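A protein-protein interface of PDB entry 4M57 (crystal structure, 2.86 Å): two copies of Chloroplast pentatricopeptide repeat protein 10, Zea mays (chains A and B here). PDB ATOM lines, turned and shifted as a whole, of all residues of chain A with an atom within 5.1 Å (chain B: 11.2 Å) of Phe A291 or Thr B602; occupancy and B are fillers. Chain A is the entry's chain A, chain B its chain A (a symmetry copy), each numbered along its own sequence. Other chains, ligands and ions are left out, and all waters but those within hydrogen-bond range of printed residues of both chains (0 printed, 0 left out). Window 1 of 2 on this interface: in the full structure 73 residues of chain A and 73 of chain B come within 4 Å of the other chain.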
ATOM      1  N   ARG A 267     -27.089  28.991  -6.054  1.00  0.00           N
ATOM      2  CA  ARG A 267     -27.746  27.686  -6.106  1.00  0.00           C
ATOM      3  C   ARG A 267     -29.262  27.758  -5.862  1.00  0.00           C
ATOM      4  O   ARG A 267     -29.984  26.835  -6.229  1.00  0.00           O
ATOM      5  CB  ARG A 267     -27.111  26.705  -5.116  1.00  0.00           C
ATOM      6  CG  ARG A 267     -25.929  25.925  -5.648  1.00  0.00           C
ATOM      7  CD  ARG A 267     -24.866  25.730  -4.574  1.00  0.00           C
ATOM      8  NE  ARG A 267     -25.467  25.660  -3.240  1.00  0.00           N
ATOM      9  CZ  ARG A 267     -24.890  26.098  -2.124  1.00  0.00           C
ATOM     10  NH1 ARG A 267     -23.670  26.641  -2.165  1.00  0.00           N
ATOM     11  NH2 ARG A 267     -25.538  25.992  -0.968  1.00  0.00           N
ATOM     12  N   ASN A 289     -13.993  32.043  -4.615  1.00  0.00           N
ATOM     13  CA  ASN A 289     -13.528  30.699  -4.902  1.00  0.00           C
ATOM     14  C   ASN A 289     -13.368  30.421  -6.387  1.00  0.00           C
ATOM     15  O   ASN A 289     -13.100  31.314  -7.180  1.00  0.00           O
ATOM     16  CB  ASN A 289     -14.504  29.682  -4.332  1.00  0.00           C
ATOM     17  CG  ASN A 289     -14.211  29.357  -2.893  1.00  0.00           C
ATOM     18  OD1 ASN A 289     -13.077  29.488  -2.452  1.00  0.00           O
ATOM     19  ND2 ASN A 289     -15.227  28.929  -2.146  1.00  0.00           N
ATOM     20  N   ALA A 290     -13.504  29.157  -6.754  1.00  0.00           N
ATOM     21  CA  ALA A 290     -13.648  28.790  -8.147  1.00  0.00           C
ATOM     22  C   ALA A 290     -15.060  28.255  -8.230  1.00  0.00           C
ATOM     23  O   ALA A 290     -15.832  28.622  -9.116  1.00  0.00           O
ATOM     24  CB  ALA A 290     -12.631  27.711  -8.546  1.00  0.00           C
ATOM     25  N   PHE A 291     -15.378  27.394  -7.272  1.00  0.00           N
ATOM     26  CA  PHE A 291     -16.676  26.761  -7.162  1.00  0.00           C
ATOM     27  C   PHE A 291     -17.809  27.778  -7.082  1.00  0.00           C
ATOM     28  O   PHE A 291     -18.910  27.540  -7.599  1.00  0.00           O
ATOM     29  CB  PHE A 291     -16.706  25.865  -5.937  1.00  0.00           C
ATOM     30  CG  PHE A 291     -18.064  25.347  -5.607  1.00  0.00           C
ATOM     31  CD1 PHE A 291     -18.513  24.153  -6.152  1.00  0.00           C
ATOM     32  CD2 PHE A 291     -18.905  26.050  -4.748  1.00  0.00           C
ATOM     33  CE1 PHE A 291     -19.776  23.675  -5.860  1.00  0.00           C
ATOM     34  CE2 PHE A 291     -20.168  25.573  -4.462  1.00  0.00           C
ATOM     35  CZ  PHE A 291     -20.600  24.383  -5.020  1.00  0.00           C
ATOM     36  N   THR A 292     -17.561  28.906  -6.427  1.00  0.00           N
ATOM     37  CA  THR A 292     -18.616  29.901  -6.328  1.00  0.00           C
ATOM     38  C   THR A 292     -18.784  30.614  -7.671  1.00  0.00           C
ATOM     39  O   THR A 292     -19.908  30.803  -8.138  1.00  0.00           O
ATOM     40  CB  THR A 292     -18.406  30.886  -5.147  1.00  0.00           C
ATOM     41  OG1 THR A 292     -17.499  31.926  -5.524  1.00  0.00           O
ATOM     42  CG2 THR A 292     -17.898  30.148  -3.904  1.00  0.00           C
ATOM     43  N   TYR A 293     -17.662  30.975  -8.295  1.00  0.00           N
ATOM     44  CA  TYR A 293     -17.651  31.527  -9.651  1.00  0.00           C
ATOM     45  C   TYR A 293     -18.464  30.632 -10.574  1.00  0.00           C
ATOM     46  O   TYR A 293     -19.294  31.103 -11.350  1.00  0.00           O
ATOM     47  CB  TYR A 293     -16.210  31.639 -10.167  1.00  0.00           C
ATOM     48  CG  TYR A 293     -15.575  33.015 -10.047  1.00  0.00           C
ATOM     49  CD1 TYR A 293     -16.314  34.161 -10.276  1.00  0.00           C
ATOM     50  CD2 TYR A 293     -14.231  33.164  -9.717  1.00  0.00           C
ATOM     51  CE1 TYR A 293     -15.744  35.421 -10.171  1.00  0.00           C
ATOM     52  CE2 TYR A 293     -13.650  34.423  -9.609  1.00  0.00           C
ATOM     53  CZ  TYR A 293     -14.417  35.550  -9.840  1.00  0.00           C
ATOM     54  OH  TYR A 293     -13.879  36.815  -9.741  1.00  0.00           O
ATOM     55  N   ASN A 294     -18.237  29.332 -10.462  1.00  0.00           N
ATOM     56  CA  ASN A 294     -18.906  28.374 -11.316  1.00  0.00           C
ATOM     57  C   ASN A 294     -20.381  28.302 -11.015  1.00  0.00           C
ATOM     58  O   ASN A 294     -21.195  28.059 -11.907  1.00  0.00           O
ATOM     59  CB  ASN A 294     -18.292  26.982 -11.164  1.00  0.00           C
ATOM     60  CG  ASN A 294     -17.374  26.619 -12.323  1.00  0.00           C
ATOM     61  OD1 ASN A 294     -17.538  27.103 -13.448  1.00  0.00           O
ATOM     62  ND2 ASN A 294     -16.391  25.770 -12.047  1.00  0.00           N
ATOM     63  N   THR A 295     -20.710  28.503  -9.744  1.00  0.00           N
ATOM     64  CA  THR A 295     -22.083  28.367  -9.276  1.00  0.00           C
ATOM     65  C   THR A 295     -22.932  29.536  -9.776  1.00  0.00           C
ATOM     66  O   THR A 295     -24.089  29.350 -10.199  1.00  0.00           O
ATOM     67  CB  THR A 295     -22.136  28.190  -7.740  1.00  0.00           C
ATOM     68  OG1 THR A 295     -21.825  26.830  -7.421  1.00  0.00           O
ATOM     69  CG2 THR A 295     -23.491  28.458  -7.212  1.00  0.00           C
ATOM     70  N   ASN A 326     -13.369  20.661 -15.830  1.00  0.00           N
ATOM     71  CA  ASN A 326     -14.751  20.606 -15.389  1.00  0.00           C
ATOM     72  C   ASN A 326     -15.423  21.943 -15.564  1.00  0.00           C
ATOM     73  O   ASN A 326     -16.609  22.022 -15.850  1.00  0.00           O
ATOM     74  CB  ASN A 326     -14.822  20.157 -13.942  1.00  0.00           C
ATOM     75  CG  ASN A 326     -14.117  18.855 -13.725  1.00  0.00           C
ATOM     76  OD1 ASN A 326     -14.034  18.042 -14.646  1.00  0.00           O
ATOM     77  ND2 ASN A 326     -13.587  18.642 -12.515  1.00  0.00           N
ATOM     78  N   THR A 327     -14.645  22.998 -15.393  1.00  0.00           N
ATOM     79  CA  THR A 327     -15.153  24.342 -15.558  1.00  0.00           C
ATOM     80  C   THR A 327     -15.438  24.606 -17.022  1.00  0.00           C
ATOM     81  O   THR A 327     -16.482  25.170 -17.366  1.00  0.00           O
ATOM     82  CB  THR A 327     -14.154  25.345 -15.020  1.00  0.00           C
ATOM     83  OG1 THR A 327     -13.803  24.945 -13.693  1.00  0.00           O
ATOM     84  CG2 THR A 327     -14.741  26.736 -14.989  1.00  0.00           C
ATOM     85  N   LEU A 330     -18.395  22.688 -18.053  1.00  0.00           N
ATOM     86  CA  LEU A 330     -19.561  23.331 -17.512  1.00  0.00           C
ATOM     87  C   LEU A 330     -20.017  24.427 -18.453  1.00  0.00           C
ATOM     88  O   LEU A 330     -21.172  24.453 -18.874  1.00  0.00           O
ATOM     89  CB  LEU A 330     -19.251  23.900 -16.133  1.00  0.00           C
ATOM     90  CG  LEU A 330     -20.513  24.247 -15.361  1.00  0.00           C
ATOM     91  CD1 LEU A 330     -20.541  23.443 -14.068  1.00  0.00           C
ATOM     92  CD2 LEU A 330     -20.617  25.759 -15.126  1.00  0.00           C
ATOM     93  N   SER B 568     -20.488  12.469 -15.832  1.00  0.00           N
ATOM     94  CA  SER B 568     -19.591  12.844 -14.729  1.00  0.00           C
ATOM     95  C   SER B 568     -20.258  12.691 -13.355  1.00  0.00           C
ATOM     96  O   SER B 568     -21.361  13.205 -13.124  1.00  0.00           O
ATOM     97  CB  SER B 568     -19.064  14.273 -14.911  1.00  0.00           C
ATOM     98  OG  SER B 568     -20.127  15.205 -15.046  1.00  0.00           O
ATOM     99  N   PRO B 569     -19.575  12.001 -12.430  1.00  0.00           N
ATOM    100  CA  PRO B 569     -20.105  11.619 -11.114  1.00  0.00           C
ATOM    101  C   PRO B 569     -20.503  12.815 -10.248  1.00  0.00           C
ATOM    102  O   PRO B 569     -19.997  13.920 -10.477  1.00  0.00           O
ATOM    103  CB  PRO B 569     -18.925  10.881 -10.472  1.00  0.00           C
ATOM    104  CG  PRO B 569     -18.057  10.470 -11.620  1.00  0.00           C
ATOM    105  CD  PRO B 569     -18.177  11.578 -12.599  1.00  0.00           C
ATOM    106  N   ASP B 570     -21.391  12.601  -9.277  1.00  0.00           N
ATOM    107  CA  ASP B 570     -21.778  13.678  -8.361  1.00  0.00           C
ATOM    108  C   ASP B 570     -21.338  13.412  -6.931  1.00  0.00           C
ATOM    109  O   ASP B 570     -20.429  12.645  -6.681  1.00  0.00           O
ATOM    110  CB  ASP B 570     -23.287  13.956  -8.404  1.00  0.00           C
ATOM    111  CG  ASP B 570     -24.118  12.705  -8.218  1.00  0.00           C
ATOM    112  OD1 ASP B 570     -23.777  11.875  -7.356  1.00  0.00           O
ATOM    113  OD2 ASP B 570     -25.125  12.548  -8.940  1.00  0.00           O
ATOM    114  N   LEU B 571     -22.001  14.053  -5.986  1.00  0.00           N
ATOM    115  CA  LEU B 571     -21.677  13.835  -4.592  1.00  0.00           C
ATOM    116  C   LEU B 571     -22.073  12.443  -4.151  1.00  0.00           C
ATOM    117  O   LEU B 571     -21.322  11.814  -3.431  1.00  0.00           O
ATOM    118  CB  LEU B 571     -22.348  14.879  -3.709  1.00  0.00           C
ATOM    119  CG  LEU B 571     -21.339  15.781  -3.016  1.00  0.00           C
ATOM    120  CD1 LEU B 571     -22.007  17.047  -2.553  1.00  0.00           C
ATOM    121  CD2 LEU B 571     -20.694  15.046  -1.850  1.00  0.00           C
ATOM    122  N   TYR B 574     -19.116  10.109  -5.188  1.00  0.00           N
ATOM    123  CA  TYR B 574     -17.869  10.265  -4.452  1.00  0.00           C
ATOM    124  C   TYR B 574     -18.026   9.890  -2.968  1.00  0.00           C
ATOM    125  O   TYR B 574     -17.086   9.411  -2.324  1.00  0.00           O
ATOM    126  CB  TYR B 574     -17.324  11.694  -4.611  1.00  0.00           C
ATOM    127  CG  TYR B 574     -16.751  12.005  -5.984  1.00  0.00           C
ATOM    128  CD1 TYR B 574     -15.486  11.563  -6.354  1.00  0.00           C
ATOM    129  CD2 TYR B 574     -17.475  12.752  -6.903  1.00  0.00           C
ATOM    130  CE1 TYR B 574     -14.966  11.845  -7.612  1.00  0.00           C
ATOM    131  CE2 TYR B 574     -16.972  13.045  -8.150  1.00  0.00           C
ATOM    132  CZ  TYR B 574     -15.717  12.593  -8.510  1.00  0.00           C
ATOM    133  OH  TYR B 574     -15.228  12.898  -9.772  1.00  0.00           O
ATOM    134  N   LEU B 594     -11.661  13.165  -0.905  1.00  0.00           N
ATOM    135  CA  LEU B 594     -12.086  14.405  -0.247  1.00  0.00           C
ATOM    136  C   LEU B 594     -11.327  15.607  -0.769  1.00  0.00           C
ATOM    137  O   LEU B 594     -11.900  16.675  -0.993  1.00  0.00           O
ATOM    138  CB  LEU B 594     -11.794  14.317   1.255  1.00  0.00           C
ATOM    139  CG  LEU B 594     -12.647  15.087   2.280  1.00  0.00           C
ATOM    140  CD1 LEU B 594     -11.795  16.029   3.138  1.00  0.00           C
ATOM    141  CD2 LEU B 594     -13.783  15.824   1.608  1.00  0.00           C
ATOM    142  N   ASN B 595     -10.018  15.431  -0.907  1.00  0.00           N
ATOM    143  CA  ASN B 595      -9.144  16.508  -1.325  1.00  0.00           C
ATOM    144  C   ASN B 595      -9.381  16.826  -2.789  1.00  0.00           C
ATOM    145  O   ASN B 595      -9.398  18.001  -3.189  1.00  0.00           O
ATOM    146  CB  ASN B 595      -7.687  16.122  -1.087  1.00  0.00           C
ATOM    147  CG  ASN B 595      -7.271  16.270   0.367  1.00  0.00           C
ATOM    148  OD1 ASN B 595      -8.100  16.285   1.280  1.00  0.00           O
ATOM    149  ND2 ASN B 595      -5.971  16.393   0.586  1.00  0.00           N
ATOM    150  N   GLN B 596      -9.578  15.770  -3.580  1.00  0.00           N
ATOM    151  CA  GLN B 596      -9.929  15.911  -4.986  1.00  0.00           C
ATOM    152  C   GLN B 596     -11.139  16.831  -5.098  1.00  0.00           C
ATOM    153  O   GLN B 596     -11.071  17.877  -5.727  1.00  0.00           O
ATOM    154  CB  GLN B 596     -10.217  14.540  -5.617  1.00  0.00           C
ATOM    155  CG  GLN B 596      -8.983  13.633  -5.779  1.00  0.00           C
ATOM    156  CD  GLN B 596      -9.314  12.186  -6.209  1.00  0.00           C
ATOM    157  OE1 GLN B 596     -10.269  11.940  -6.958  1.00  0.00           O
ATOM    158  NE2 GLN B 596      -8.512  11.229  -5.730  1.00  0.00           N
ATOM    159  N   LEU B 597     -12.234  16.439  -4.456  1.00  0.00           N
ATOM    160  CA  LEU B 597     -13.421  17.273  -4.348  1.00  0.00           C
ATOM    161  C   LEU B 597     -13.104  18.686  -3.913  1.00  0.00           C
ATOM    162  O   LEU B 597     -13.696  19.638  -4.405  1.00  0.00           O
ATOM    163  CB  LEU B 597     -14.381  16.676  -3.332  1.00  0.00           C
ATOM    164  CG  LEU B 597     -15.072  15.401  -3.775  1.00  0.00           C
ATOM    165  CD1 LEU B 597     -15.637  14.726  -2.558  1.00  0.00           C
ATOM    166  CD2 LEU B 597     -16.187  15.714  -4.749  1.00  0.00           C
ATOM    167  N   LYS B 598     -12.191  18.822  -2.964  1.00  0.00           N
ATOM    168  CA  LYS B 598     -11.881  20.133  -2.418  1.00  0.00           C
ATOM    169  C   LYS B 598     -11.409  21.050  -3.524  1.00  0.00           C
ATOM    170  O   LYS B 598     -11.803  22.217  -3.589  1.00  0.00           O
ATOM    171  CB  LYS B 598     -10.834  20.039  -1.320  1.00  0.00           C
ATOM    172  CG  LYS B 598     -11.379  20.332   0.048  1.00  0.00           C
ATOM    173  CD  LYS B 598     -10.403  19.881   1.119  1.00  0.00           C
ATOM    174  CE  LYS B 598     -10.910  20.234   2.511  1.00  0.00           C
ATOM    175  NZ  LYS B 598     -10.820  21.692   2.813  1.00  0.00           N
ATOM    176  N   CYS B 599     -10.583  20.523  -4.416  1.00  0.00           N
ATOM    177  CA  CYS B 599     -10.110  21.365  -5.510  1.00  0.00           C
ATOM    178  C   CYS B 599     -10.695  20.963  -6.861  1.00  0.00           C
ATOM    179  O   CYS B 599     -10.011  20.990  -7.877  1.00  0.00           O
ATOM    180  CB  CYS B 599      -8.580  21.400  -5.549  1.00  0.00           C
ATOM    181  SG  CYS B 599      -7.810  19.781  -5.702  1.00  0.00           S
ATOM    182  N   SER B 600     -11.980  20.627  -6.856  1.00  0.00           N
ATOM    183  CA  SER B 600     -12.684  20.159  -8.043  1.00  0.00           C
ATOM    184  C   SER B 600     -13.082  21.319  -8.968  1.00  0.00           C
ATOM    185  O   SER B 600     -13.179  21.142 -10.195  1.00  0.00           O
ATOM    186  CB  SER B 600     -13.926  19.369  -7.617  1.00  0.00           C
ATOM    187  OG  SER B 600     -14.478  18.629  -8.693  1.00  0.00           O
ATOM    188  N   GLN B 601     -13.308  22.486  -8.364  1.00  0.00           N
ATOM    189  CA  GLN B 601     -13.745  23.712  -9.049  1.00  0.00           C
ATOM    190  C   GLN B 601     -15.245  23.723  -9.351  1.00  0.00           C
ATOM    191  O   GLN B 601     -15.840  24.780  -9.489  1.00  0.00           O
ATOM    192  CB  GLN B 601     -12.939  24.018 -10.323  1.00  0.00           C
ATOM    193  CG  GLN B 601     -11.510  24.468 -10.098  1.00  0.00           C
ATOM    194  CD  GLN B 601     -10.849  25.042 -11.356  1.00  0.00           C
ATOM    195  OE1 GLN B 601     -11.408  24.989 -12.439  1.00  0.00           O
ATOM    196  NE2 GLN B 601      -9.660  25.597 -11.199  1.00  0.00           N
ATOM    197  N   THR B 602     -15.856  22.549  -9.435  1.00  0.00           N
ATOM    198  CA  THR B 602     -17.245  22.479  -9.826  1.00  0.00           C
ATOM    199  C   THR B 602     -18.065  21.751  -8.797  1.00  0.00           C
ATOM    200  O   THR B 602     -19.292  21.815  -8.819  1.00  0.00           O
ATOM    201  CB  THR B 602     -17.413  21.774 -11.177  1.00  0.00           C
ATOM    202  OG1 THR B 602     -16.581  20.613 -11.219  1.00  0.00           O
ATOM    203  CG2 THR B 602     -17.020  22.699 -12.306  1.00  0.00           C
ATOM    204  N   MET B 603     -17.380  21.033  -7.910  1.00  0.00           N
ATOM    205  CA  MET B 603     -18.035  20.350  -6.809  1.00  0.00           C
ATOM    206  C   MET B 603     -17.379  20.804  -5.525  1.00  0.00           C
ATOM    207  O   MET B 603     -16.189  21.143  -5.519  1.00  0.00           O
ATOM    208  CB  MET B 603     -17.884  18.834  -6.920  1.00  0.00           C
ATOM    209  CG  MET B 603     -18.026  18.279  -8.305  1.00  0.00           C
ATOM    210  SD  MET B 603     -18.671  16.601  -8.333  1.00  0.00           S
ATOM    211  CE  MET B 603     -20.424  16.919  -8.387  1.00  0.00           C
ATOM    212  N   LYS B 604     -18.154  20.828  -4.443  1.00  0.00           N
ATOM    213  CA  LYS B 604     -17.574  20.877  -3.104  1.00  0.00           C
ATOM    214  C   LYS B 604     -18.095  19.687  -2.329  1.00  0.00           C
ATOM    215  O   LYS B 604     -19.125  19.118  -2.689  1.00  0.00           O
ATOM    216  CB  LYS B 604     -17.875  22.197  -2.385  1.00  0.00           C
ATOM    217  CG  LYS B 604     -19.259  22.338  -1.838  1.00  0.00           C
ATOM    218  CD  LYS B 604     -19.463  23.753  -1.275  1.00  0.00           C
ATOM    219  CE  LYS B 604     -19.616  23.778   0.264  1.00  0.00           C
ATOM    220  NZ  LYS B 604     -20.866  23.106   0.782  1.00  0.00           N
ATOM    221  N   PRO B 605     -17.362  19.268  -1.291  1.00  0.00           N
ATOM    222  CA  PRO B 605     -17.849  18.196  -0.420  1.00  0.00           C
ATOM    223  C   PRO B 605     -18.842  18.747   0.597  1.00  0.00           C
ATOM    224  O   PRO B 605     -18.776  19.922   0.968  1.00  0.00           O
ATOM    225  CB  PRO B 605     -16.586  17.731   0.312  1.00  0.00           C
ATOM    226  CG  PRO B 605     -15.458  18.441  -0.308  1.00  0.00           C
ATOM    227  CD  PRO B 605     -15.994  19.667  -0.945  1.00  0.00           C
ATOM    228  N   ASP B 606     -19.769  17.913   1.043  1.00  0.00           N
ATOM    229  CA  ASP B 606     -20.668  18.356   2.094  1.00  0.00           C
ATOM    230  C   ASP B 606     -20.402  17.619   3.397  1.00  0.00           C
ATOM    231  O   ASP B 606     -19.469  16.827   3.485  1.00  0.00           O
ATOM    232  CB  ASP B 606     -22.135  18.257   1.661  1.00  0.00           C
ATOM    233  CG  ASP B 606     -22.521  16.873   1.159  1.00  0.00           C
ATOM    234  OD1 ASP B 606     -22.111  15.859   1.772  1.00  0.00           O
ATOM    235  OD2 ASP B 606     -23.253  16.808   0.145  1.00  0.00           O
ATOM    236  N   TYR B 610     -17.120  14.688   4.831  1.00  0.00           N
ATOM    237  CA  TYR B 610     -16.278  14.941   6.008  1.00  0.00           C
ATOM    238  C   TYR B 610     -16.527  13.920   7.128  1.00  0.00           C
ATOM    239  O   TYR B 610     -15.599  13.284   7.595  1.00  0.00           O
ATOM    240  CB  TYR B 610     -16.456  16.362   6.541  1.00  0.00           C
ATOM    241  CG  TYR B 610     -15.908  17.445   5.648  1.00  0.00           C
ATOM    242  CD1 TYR B 610     -14.549  17.737   5.619  1.00  0.00           C
ATOM    243  CD2 TYR B 610     -16.759  18.189   4.844  1.00  0.00           C
ATOM    244  CE1 TYR B 610     -14.051  18.737   4.805  1.00  0.00           C
ATOM    245  CE2 TYR B 610     -16.279  19.191   4.028  1.00  0.00           C
ATOM    246  CZ  TYR B 610     -14.925  19.464   4.011  1.00  0.00           C
ATOM    247  OH  TYR B 610     -14.466  20.475   3.187  1.00  0.00           O
ATOM    248  N   ASP B 636     -13.435  25.353   6.292  1.00  0.00           N
ATOM    249  CA  ASP B 636     -14.209  25.682   5.092  1.00  0.00           C
ATOM    250  C   ASP B 636     -15.655  25.975   5.472  1.00  0.00           C
ATOM    251  O   ASP B 636     -16.561  25.881   4.635  1.00  0.00           O
ATOM    252  CB  ASP B 636     -14.177  24.548   4.064  1.00  0.00           C
ATOM    253  CG  ASP B 636     -12.840  23.835   4.016  1.00  0.00           C
ATOM    254  OD1 ASP B 636     -11.789  24.516   4.071  1.00  0.00           O
ATOM    255  OD2 ASP B 636     -12.841  22.584   3.935  1.00  0.00           O
ATOM    256  N   MET B 638     -17.822  24.513   7.517  1.00  0.00           N
ATOM    257  CA  MET B 638     -18.771  23.447   7.799  1.00  0.00           C
ATOM    258  C   MET B 638     -18.909  23.200   9.304  1.00  0.00           C
ATOM    259  O   MET B 638     -17.911  23.171  10.047  1.00  0.00           O
ATOM    260  CB  MET B 638     -18.341  22.165   7.104  1.00  0.00           C
ATOM    261  CG  MET B 638     -19.468  21.416   6.495  1.00  0.00           C
ATOM    262  SD  MET B 638     -19.453  21.699   4.739  1.00  0.00           S
ATOM    263  CE  MET B 638     -21.210  21.572   4.407  1.00  0.00           C
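The backbone NH (N) of Phe A291 lies close to the backbone carbonyl oxygen (O) of Gln B601, 3.5 Å away. The side-chain amide nitrogen of Asn A294 lies within hydrogen-bond range of the backbone carbonyl oxygen of Gln B601 (2.8 Å). ND2 of Asn A326 is in hydrogen-bond range of O of Ser B600, at 3.4 Å. The side-chain hydroxyl of Thr A327 sits at hydrogen-bond distance from the side-chain amide oxygen of Gln B601, 2.7 Å away.
Ala A290 touches Gln B601. CE1 of Phe A291 touches O of Thr B602, 3.5 Å away. Phe A291 touches Met B603. Phe A291 touches Lys B604. Thr B602 touches Asn A294. Asn A326 touches Thr B602. Thr B602 touches Thr A327 (CG2 to N, 3.9 Å).
Printed residues of chain B that touch a printed residue of chain A: Ser B600, Gln B601, Thr B602, Met B603 and Lys B604. Of the 11 printed residues of chain A, 5 touch a printed residue of chain B. Hydrophobic or aromatic side chains of chain A within 4 Å of the printed part of chain B: Ala A290 and Phe A291.
No residue of chain B comes within 4 Å of Asn A289. Ala A290 touches one residue of chain B. No residue of chain B comes within 4 Å of Thr A295. Asn B595 touches none of the printed residues of chain A. Printed residues of chain A within 4 Å of Ser B600: Asn A326 (3.4 Å). Of the printed residues of chain A, Gln B601 touches Ala A290 (3.8 Å), Phe A291 (3.2 Å), Asn A294 (2.8 Å) and Thr A327 (2.7 Å). Of the printed residues of chain A, Thr B602 touches Phe A291 (3.5 Å), Asn A294 (3.1 Å), Asn A326 (3.3 Å) and Thr A327 (3.9 Å). Of the printed residues of chain A, Met B603 touches Phe A291 (3.6 Å). Printed residues of chain A within 4 Å of Lys B604: Phe A291 (3.6 Å).
No position is printed for both chains.
The side-chain hydroxyl (OG1) of Thr A295 sits at hydrogen-bond distance from the backbone carbonyl oxygen (O) of Phe A291 (3.0 Å). ND2 of Asn A294 lies within hydrogen-bond range of OG1 of Thr A327 (3.2 Å).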
